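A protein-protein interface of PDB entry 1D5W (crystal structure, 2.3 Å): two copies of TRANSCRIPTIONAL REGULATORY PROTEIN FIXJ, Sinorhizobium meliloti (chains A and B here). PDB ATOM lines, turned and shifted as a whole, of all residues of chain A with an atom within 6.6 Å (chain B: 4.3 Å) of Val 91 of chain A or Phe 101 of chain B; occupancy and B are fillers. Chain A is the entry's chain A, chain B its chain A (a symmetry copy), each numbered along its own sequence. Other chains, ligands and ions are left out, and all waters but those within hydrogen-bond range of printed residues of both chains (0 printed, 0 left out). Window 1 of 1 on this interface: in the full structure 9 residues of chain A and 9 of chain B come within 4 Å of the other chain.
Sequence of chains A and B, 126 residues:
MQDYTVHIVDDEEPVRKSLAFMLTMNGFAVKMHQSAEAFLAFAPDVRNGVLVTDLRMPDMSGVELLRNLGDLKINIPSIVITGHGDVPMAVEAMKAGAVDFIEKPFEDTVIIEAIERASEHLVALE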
ATOM      1  N   ASP A  86      18.991  10.117 -22.359  1.00  0.00           N
ATOM      2  CA  ASP A  86      18.810  10.216 -23.806  1.00  0.00           C
ATOM      3  C   ASP A  86      19.185   8.867 -24.420  1.00  0.00           C
ATOM      4  O   ASP A  86      19.752   7.986 -23.741  1.00  0.00           O
ATOM      5  CB  ASP A  86      19.647  11.356 -24.418  1.00  0.00           C
ATOM      6  CG  ASP A  86      21.129  11.244 -24.102  1.00  0.00           C
ATOM      7  OD1 ASP A  86      21.675  10.115 -24.101  1.00  0.00           O
ATOM      8  OD2 ASP A  86      21.761  12.296 -23.868  1.00  0.00           O
ATOM      9  N   VAL A  87      18.869   8.694 -25.698  1.00  0.00           N
ATOM     10  CA  VAL A  87      19.150   7.427 -26.363  1.00  0.00           C
ATOM     11  C   VAL A  87      20.600   6.963 -26.242  1.00  0.00           C
ATOM     12  O   VAL A  87      20.868   5.829 -25.823  1.00  0.00           O
ATOM     13  CB  VAL A  87      18.750   7.485 -27.858  1.00  0.00           C
ATOM     14  CG1 VAL A  87      19.315   6.269 -28.606  1.00  0.00           C
ATOM     15  CG2 VAL A  87      17.222   7.519 -27.978  1.00  0.00           C
ATOM     16  N   PRO A  88      21.555   7.831 -26.604  1.00  0.00           N
ATOM     17  CA  PRO A  88      22.983   7.477 -26.529  1.00  0.00           C
ATOM     18  C   PRO A  88      23.393   6.971 -25.146  1.00  0.00           C
ATOM     19  O   PRO A  88      24.016   5.916 -25.020  1.00  0.00           O
ATOM     20  CB  PRO A  88      23.677   8.776 -26.901  1.00  0.00           C
ATOM     21  CG  PRO A  88      22.677   9.420 -27.834  1.00  0.00           C
ATOM     22  CD  PRO A  88      21.377   9.200 -27.118  1.00  0.00           C
ATOM     23  N   MET A  89      23.032   7.724 -24.110  1.00  0.00           N
ATOM     24  CA  MET A  89      23.355   7.329 -22.743  1.00  0.00           C
ATOM     25  C   MET A  89      22.720   5.988 -22.399  1.00  0.00           C
ATOM     26  O   MET A  89      23.376   5.097 -21.841  1.00  0.00           O
ATOM     27  CB  MET A  89      22.879   8.398 -21.766  1.00  0.00           C
ATOM     28  CG  MET A  89      23.905   9.489 -21.535  1.00  0.00           C
ATOM     29  SD  MET A  89      25.455   8.775 -20.901  1.00  0.00           S
ATOM     30  CE  MET A  89      26.644   9.655 -21.895  1.00  0.00           C
ATOM     31  N   ALA A  90      21.441   5.849 -22.745  1.00  0.00           N
ATOM     32  CA  ALA A  90      20.701   4.617 -22.491  1.00  0.00           C
ATOM     33  C   ALA A  90      21.404   3.418 -23.145  1.00  0.00           C
ATOM     34  O   ALA A  90      21.482   2.329 -22.554  1.00  0.00           O
ATOM     35  CB  ALA A  90      19.272   4.756 -23.018  1.00  0.00           C
ATOM     36  N   VAL A  91      21.925   3.616 -24.357  1.00  0.00           N
ATOM     37  CA  VAL A  91      22.624   2.535 -25.051  1.00  0.00           C
ATOM     38  C   VAL A  91      23.951   2.242 -24.357  1.00  0.00           C
ATOM     39  O   VAL A  91      24.326   1.078 -24.194  1.00  0.00           O
ATOM     40  CB  VAL A  91      22.874   2.869 -26.556  1.00  0.00           C
ATOM     41  CG1 VAL A  91      23.835   1.827 -27.166  1.00  0.00           C
ATOM     42  CG2 VAL A  91      21.533   2.855 -27.328  1.00  0.00           C
ATOM     43  N   GLU A  92      24.665   3.290 -23.947  1.00  0.00           N
ATOM     44  CA  GLU A  92      25.932   3.100 -23.228  1.00  0.00           C
ATOM     45  C   GLU A  92      25.683   2.296 -21.944  1.00  0.00           C
ATOM     46  O   GLU A  92      26.433   1.372 -21.618  1.00  0.00           O
ATOM     47  CB  GLU A  92      26.567   4.450 -22.872  1.00  0.00           C
ATOM     48  CG  GLU A  92      27.167   5.197 -24.066  1.00  0.00           C
ATOM     49  CD  GLU A  92      27.697   6.580 -23.694  1.00  0.00           C
ATOM     50  OE1 GLU A  92      28.523   6.668 -22.758  1.00  0.00           O
ATOM     51  OE2 GLU A  92      27.292   7.579 -24.338  1.00  0.00           O
ATOM     52  N   ALA A  93      24.612   2.633 -21.230  1.00  0.00           N
ATOM     53  CA  ALA A  93      24.288   1.928 -19.995  1.00  0.00           C
ATOM     54  C   ALA A  93      24.046   0.443 -20.246  1.00  0.00           C
ATOM     55  O   ALA A  93      24.584  -0.409 -19.526  1.00  0.00           O
ATOM     56  CB  ALA A  93      23.061   2.552 -19.341  1.00  0.00           C
ATOM     57  N   MET A  94      23.231   0.117 -21.249  1.00  0.00           N
ATOM     58  CA  MET A  94      22.981  -1.296 -21.537  1.00  0.00           C
ATOM     59  C   MET A  94      24.286  -1.975 -21.998  1.00  0.00           C
ATOM     60  O   MET A  94      24.545  -3.137 -21.664  1.00  0.00           O
ATOM     61  CB  MET A  94      21.906  -1.451 -22.615  1.00  0.00           C
ATOM     62  CG  MET A  94      20.576  -0.785 -22.292  1.00  0.00           C
ATOM     63  SD  MET A  94      19.902  -1.211 -20.672  1.00  0.00           S
ATOM     64  CE  MET A  94      19.262  -2.859 -20.978  1.00  0.00           C
ATOM     65  N   LYS A  95      25.102  -1.243 -22.755  1.00  0.00           N
ATOM     66  CA  LYS A  95      26.369  -1.777 -23.247  1.00  0.00           C
ATOM     67  C   LYS A  95      27.295  -2.059 -22.070  1.00  0.00           C
ATOM     68  O   LYS A  95      28.080  -3.015 -22.098  1.00  0.00           O
ATOM     69  CB  LYS A  95      27.048  -0.787 -24.207  1.00  0.00           C
ATOM     70  CG  LYS A  95      26.528  -0.820 -25.643  1.00  0.00           C
ATOM     71  CD  LYS A  95      27.323   0.142 -26.530  1.00  0.00           C
ATOM     72  CE  LYS A  95      26.857   0.094 -27.991  1.00  0.00           C
ATOM     73  NZ  LYS A  95      27.529   1.133 -28.844  1.00  0.00           N
ATOM     74  N   ALA A  96      27.203  -1.225 -21.037  1.00  0.00           N
ATOM     75  CA  ALA A  96      28.028  -1.418 -19.856  1.00  0.00           C
ATOM     76  C   ALA A  96      27.475  -2.568 -19.008  1.00  0.00           C
ATOM     77  O   ALA A  96      28.074  -2.947 -17.995  1.00  0.00           O
ATOM     78  CB  ALA A  96      28.093  -0.128 -19.039  1.00  0.00           C
ATOM     79  N   PHE A 101      17.421   0.771 -17.813  1.00  0.00           N
ATOM     80  CA  PHE A 101      17.681   2.199 -17.793  1.00  0.00           C
ATOM     81  C   PHE A 101      16.274   2.779 -17.823  1.00  0.00           C
ATOM     82  O   PHE A 101      15.577   2.658 -18.827  1.00  0.00           O
ATOM     83  CB  PHE A 101      18.451   2.559 -19.062  1.00  0.00           C
ATOM     84  CG  PHE A 101      18.824   4.002 -19.174  1.00  0.00           C
ATOM     85  CD1 PHE A 101      20.098   4.428 -18.814  1.00  0.00           C
ATOM     86  CD2 PHE A 101      17.923   4.922 -19.709  1.00  0.00           C
ATOM     87  CE1 PHE A 101      20.481   5.748 -18.994  1.00  0.00           C
ATOM     88  CE2 PHE A 101      18.292   6.244 -19.892  1.00  0.00           C
ATOM     89  CZ  PHE A 101      19.581   6.663 -19.536  1.00  0.00           C
ATOM     90  N   LEU B  55      13.543   1.097 -37.533  1.00  0.00           N
ATOM     91  CA  LEU B  55      12.727   0.839 -36.347  1.00  0.00           C
ATOM     92  C   LEU B  55      11.210   0.865 -36.591  1.00  0.00           C
ATOM     93  O   LEU B  55      10.511  -0.127 -36.336  1.00  0.00           O
ATOM     94  CB  LEU B  55      13.067   1.866 -35.258  1.00  0.00           C
ATOM     95  CG  LEU B  55      12.768   1.640 -33.767  1.00  0.00           C
ATOM     96  CD1 LEU B  55      12.211   2.930 -33.220  1.00  0.00           C
ATOM     97  CD2 LEU B  55      11.807   0.501 -33.522  1.00  0.00           C
ATOM     98  N   VAL B  80      19.924  -1.401 -34.959  1.00  0.00           N
ATOM     99  CA  VAL B  80      18.670  -0.756 -35.278  1.00  0.00           C
ATOM    100  C   VAL B  80      18.991   0.694 -35.581  1.00  0.00           C
ATOM    101  O   VAL B  80      19.764   1.312 -34.853  1.00  0.00           O
ATOM    102  CB  VAL B  80      17.698  -0.783 -34.087  1.00  0.00           C
ATOM    103  CG1 VAL B  80      16.399  -0.058 -34.455  1.00  0.00           C
ATOM    104  CG2 VAL B  80      17.425  -2.212 -33.671  1.00  0.00           C
ATOM    105  N   THR B  82      17.135   4.491 -36.623  1.00  0.00           N
ATOM    106  CA  THR B  82      15.823   5.125 -36.638  1.00  0.00           C
ATOM    107  C   THR B  82      15.876   6.640 -36.502  1.00  0.00           C
ATOM    108  O   THR B  82      16.771   7.207 -35.852  1.00  0.00           O
ATOM    109  CB  THR B  82      14.964   4.597 -35.474  1.00  0.00           C
ATOM    110  OG1 THR B  82      13.620   5.087 -35.594  1.00  0.00           O
ATOM    111  CG2 THR B  82      15.546   5.085 -34.127  1.00  0.00           C
ATOM    112  N   GLY B  85      13.288   7.369 -32.663  1.00  0.00           N
ATOM    113  CA  GLY B  85      13.490   6.510 -31.511  1.00  0.00           C
ATOM    114  C   GLY B  85      13.282   7.254 -30.203  1.00  0.00           C
ATOM    115  O   GLY B  85      12.966   8.446 -30.186  1.00  0.00           O
ATOM    116  N   MET B  89      12.315   2.495 -26.347  1.00  0.00           N
ATOM    117  CA  MET B  89      12.551   1.663 -27.521  1.00  0.00           C
ATOM    118  C   MET B  89      14.003   1.209 -27.585  1.00  0.00           C
ATOM    119  O   MET B  89      14.291   0.026 -27.818  1.00  0.00           O
ATOM    120  CB  MET B  89      12.189   2.433 -28.786  1.00  0.00           C
ATOM    121  CG  MET B  89      10.728   2.297 -29.167  1.00  0.00           C
ATOM    122  SD  MET B  89      10.301   0.545 -29.415  1.00  0.00           S
ATOM    123  CE  MET B  89       8.747   0.467 -28.546  1.00  0.00           C
ATOM    124  N   ALA B  90      14.914   2.155 -27.365  1.00  0.00           N
ATOM    125  CA  ALA B  90      16.345   1.869 -27.382  1.00  0.00           C
ATOM    126  C   ALA B  90      16.690   0.768 -26.368  1.00  0.00           C
ATOM    127  O   ALA B  90      17.511  -0.119 -26.650  1.00  0.00           O
ATOM    128  CB  ALA B  90      17.130   3.146 -27.076  1.00  0.00           C
ATOM    129  N   ALA B  93      15.363  -2.580 -27.636  1.00  0.00           N
ATOM    130  CA  ALA B  93      16.242  -3.093 -28.681  1.00  0.00           C
ATOM    131  C   ALA B  93      17.471  -3.778 -28.091  1.00  0.00           C
ATOM    132  O   ALA B  93      17.827  -4.890 -28.503  1.00  0.00           O
ATOM    133  CB  ALA B  93      16.670  -1.963 -29.609  1.00  0.00           C
ATOM    134  N   MET B  94      18.136  -3.124 -27.139  1.00  0.00           N
ATOM    135  CA  MET B  94      19.314  -3.747 -26.532  1.00  0.00           C
ATOM    136  C   MET B  94      18.897  -5.018 -25.766  1.00  0.00           C
ATOM    137  O   MET B  94      19.622  -6.019 -25.761  1.00  0.00           O
ATOM    138  CB  MET B  94      20.017  -2.775 -25.582  1.00  0.00           C
ATOM    139  CG  MET B  94      20.444  -1.458 -26.215  1.00  0.00           C
ATOM    140  SD  MET B  94      21.394  -1.637 -27.741  1.00  0.00           S
ATOM    141  CE  MET B  94      23.001  -2.114 -27.103  1.00  0.00           C
ATOM    142  N   ASP B 100      23.645  -2.483 -31.206  1.00  0.00           N
ATOM    143  CA  ASP B 100      23.557  -1.032 -31.159  1.00  0.00           C
ATOM    144  C   ASP B 100      22.223  -0.513 -31.698  1.00  0.00           C
ATOM    145  O   ASP B 100      21.514  -1.189 -32.462  1.00  0.00           O
ATOM    146  CB  ASP B 100      24.720  -0.419 -31.942  1.00  0.00           C
ATOM    147  CG  ASP B 100      25.151   0.932 -31.387  1.00  0.00           C
ATOM    148  OD1 ASP B 100      26.313   1.326 -31.650  1.00  0.00           O
ATOM    149  OD2 ASP B 100      24.336   1.599 -30.697  1.00  0.00           O
ATOM    150  N   PHE B 101      21.905   0.706 -31.277  1.00  0.00           N
ATOM    151  CA  PHE B 101      20.680   1.400 -31.628  1.00  0.00           C
ATOM    152  C   PHE B 101      21.181   2.810 -31.909  1.00  0.00           C
ATOM    153  O   PHE B 101      21.617   3.504 -30.995  1.00  0.00           O
ATOM    154  CB  PHE B 101      19.756   1.378 -30.412  1.00  0.00           C
ATOM    155  CG  PHE B 101      18.429   2.031 -30.628  1.00  0.00           C
ATOM    156  CD1 PHE B 101      17.310   1.263 -30.934  1.00  0.00           C
ATOM    157  CD2 PHE B 101      18.284   3.406 -30.452  1.00  0.00           C
ATOM    158  CE1 PHE B 101      16.060   1.849 -31.052  1.00  0.00           C
ATOM    159  CE2 PHE B 101      17.041   4.005 -30.569  1.00  0.00           C
ATOM    160  CZ  PHE B 101      15.918   3.223 -30.868  1.00  0.00           C
ATOM    161  N   ILE B 102      21.116   3.232 -33.167  1.00  0.00           N
ATOM    162  CA  ILE B 102      21.640   4.530 -33.543  1.00  0.00           C
ATOM    163  C   ILE B 102      20.615   5.443 -34.170  1.00  0.00           C
ATOM    164  O   ILE B 102      19.832   5.013 -35.023  1.00  0.00           O
ATOM    165  CB  ILE B 102      22.787   4.359 -34.534  1.00  0.00           C
ATOM    166  CG1 ILE B 102      23.756   3.290 -34.008  1.00  0.00           C
ATOM    167  CG2 ILE B 102      23.482   5.699 -34.758  1.00  0.00           C
ATOM    168  CD1 ILE B 102      24.890   2.934 -34.974  1.00  0.00           C
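OD1 of Asp 100 of chain B is in salt-bridge range of NZ of Lys 95 of chain A (3.1 Å).
The backbone NH (N) of Val 80 of chain B is in hydrogen-bond range of the backbone carbonyl oxygen (O) of Asp 100 of chain B (3.0 Å).
Among the printed residues, pairs that only touch across the chains: Val 87 of chain A with Phe 101 of chain B (3.6 Å), Val 91 of chain A with Asp 100 of chain B (3.6 Å), Val 91 of chain A with Phe 101 of chain B (3.7 Å) and Met 94 of chain A with Met 94 of chain B (3.8 Å).
Printed residues of chain B within 4 Å of Val 91 of chain A: Asp 100 and Phe 101.
Of the printed residues of chain B, Met 94 of chain A touches Met 94.
Of the printed residues of chain A, Asp 100 of chain B touches Val 91 (3.6 Å) and Lys 95 (3.1 Å).
Printed residues of chain A within 4 Å of Phe 101 of chain B: Val 87 and Val 91.
The nearest residue of chain B that does not touch Val 91 of chain A is Met 94 of chain B (4.03 Å).
The nearest printed residue of chain B that does not touch Val 87 of chain A is Ala 90 of chain B (4.1 Å).
Of the 12 printed residues of chain A, 4 touch a printed residue of chain B.
Printed residues of chain A that touch a printed residue of chain B: Val 87, Val 91, Met 94 and Lys 95.
Printed residues of chain B that touch a printed residue of chain A: Met 94, Asp 100 and Phe 101.
Among the printed residues, Asp or Glu carboxylates within 4 Å of a Lys or Arg side-chain nitrogen of the other chain: Lys 95 of chain A with Asp 100 of chain B (3.1 Å).
Met 94 of chain B touches its own counterpart, Met 94 of chain A.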
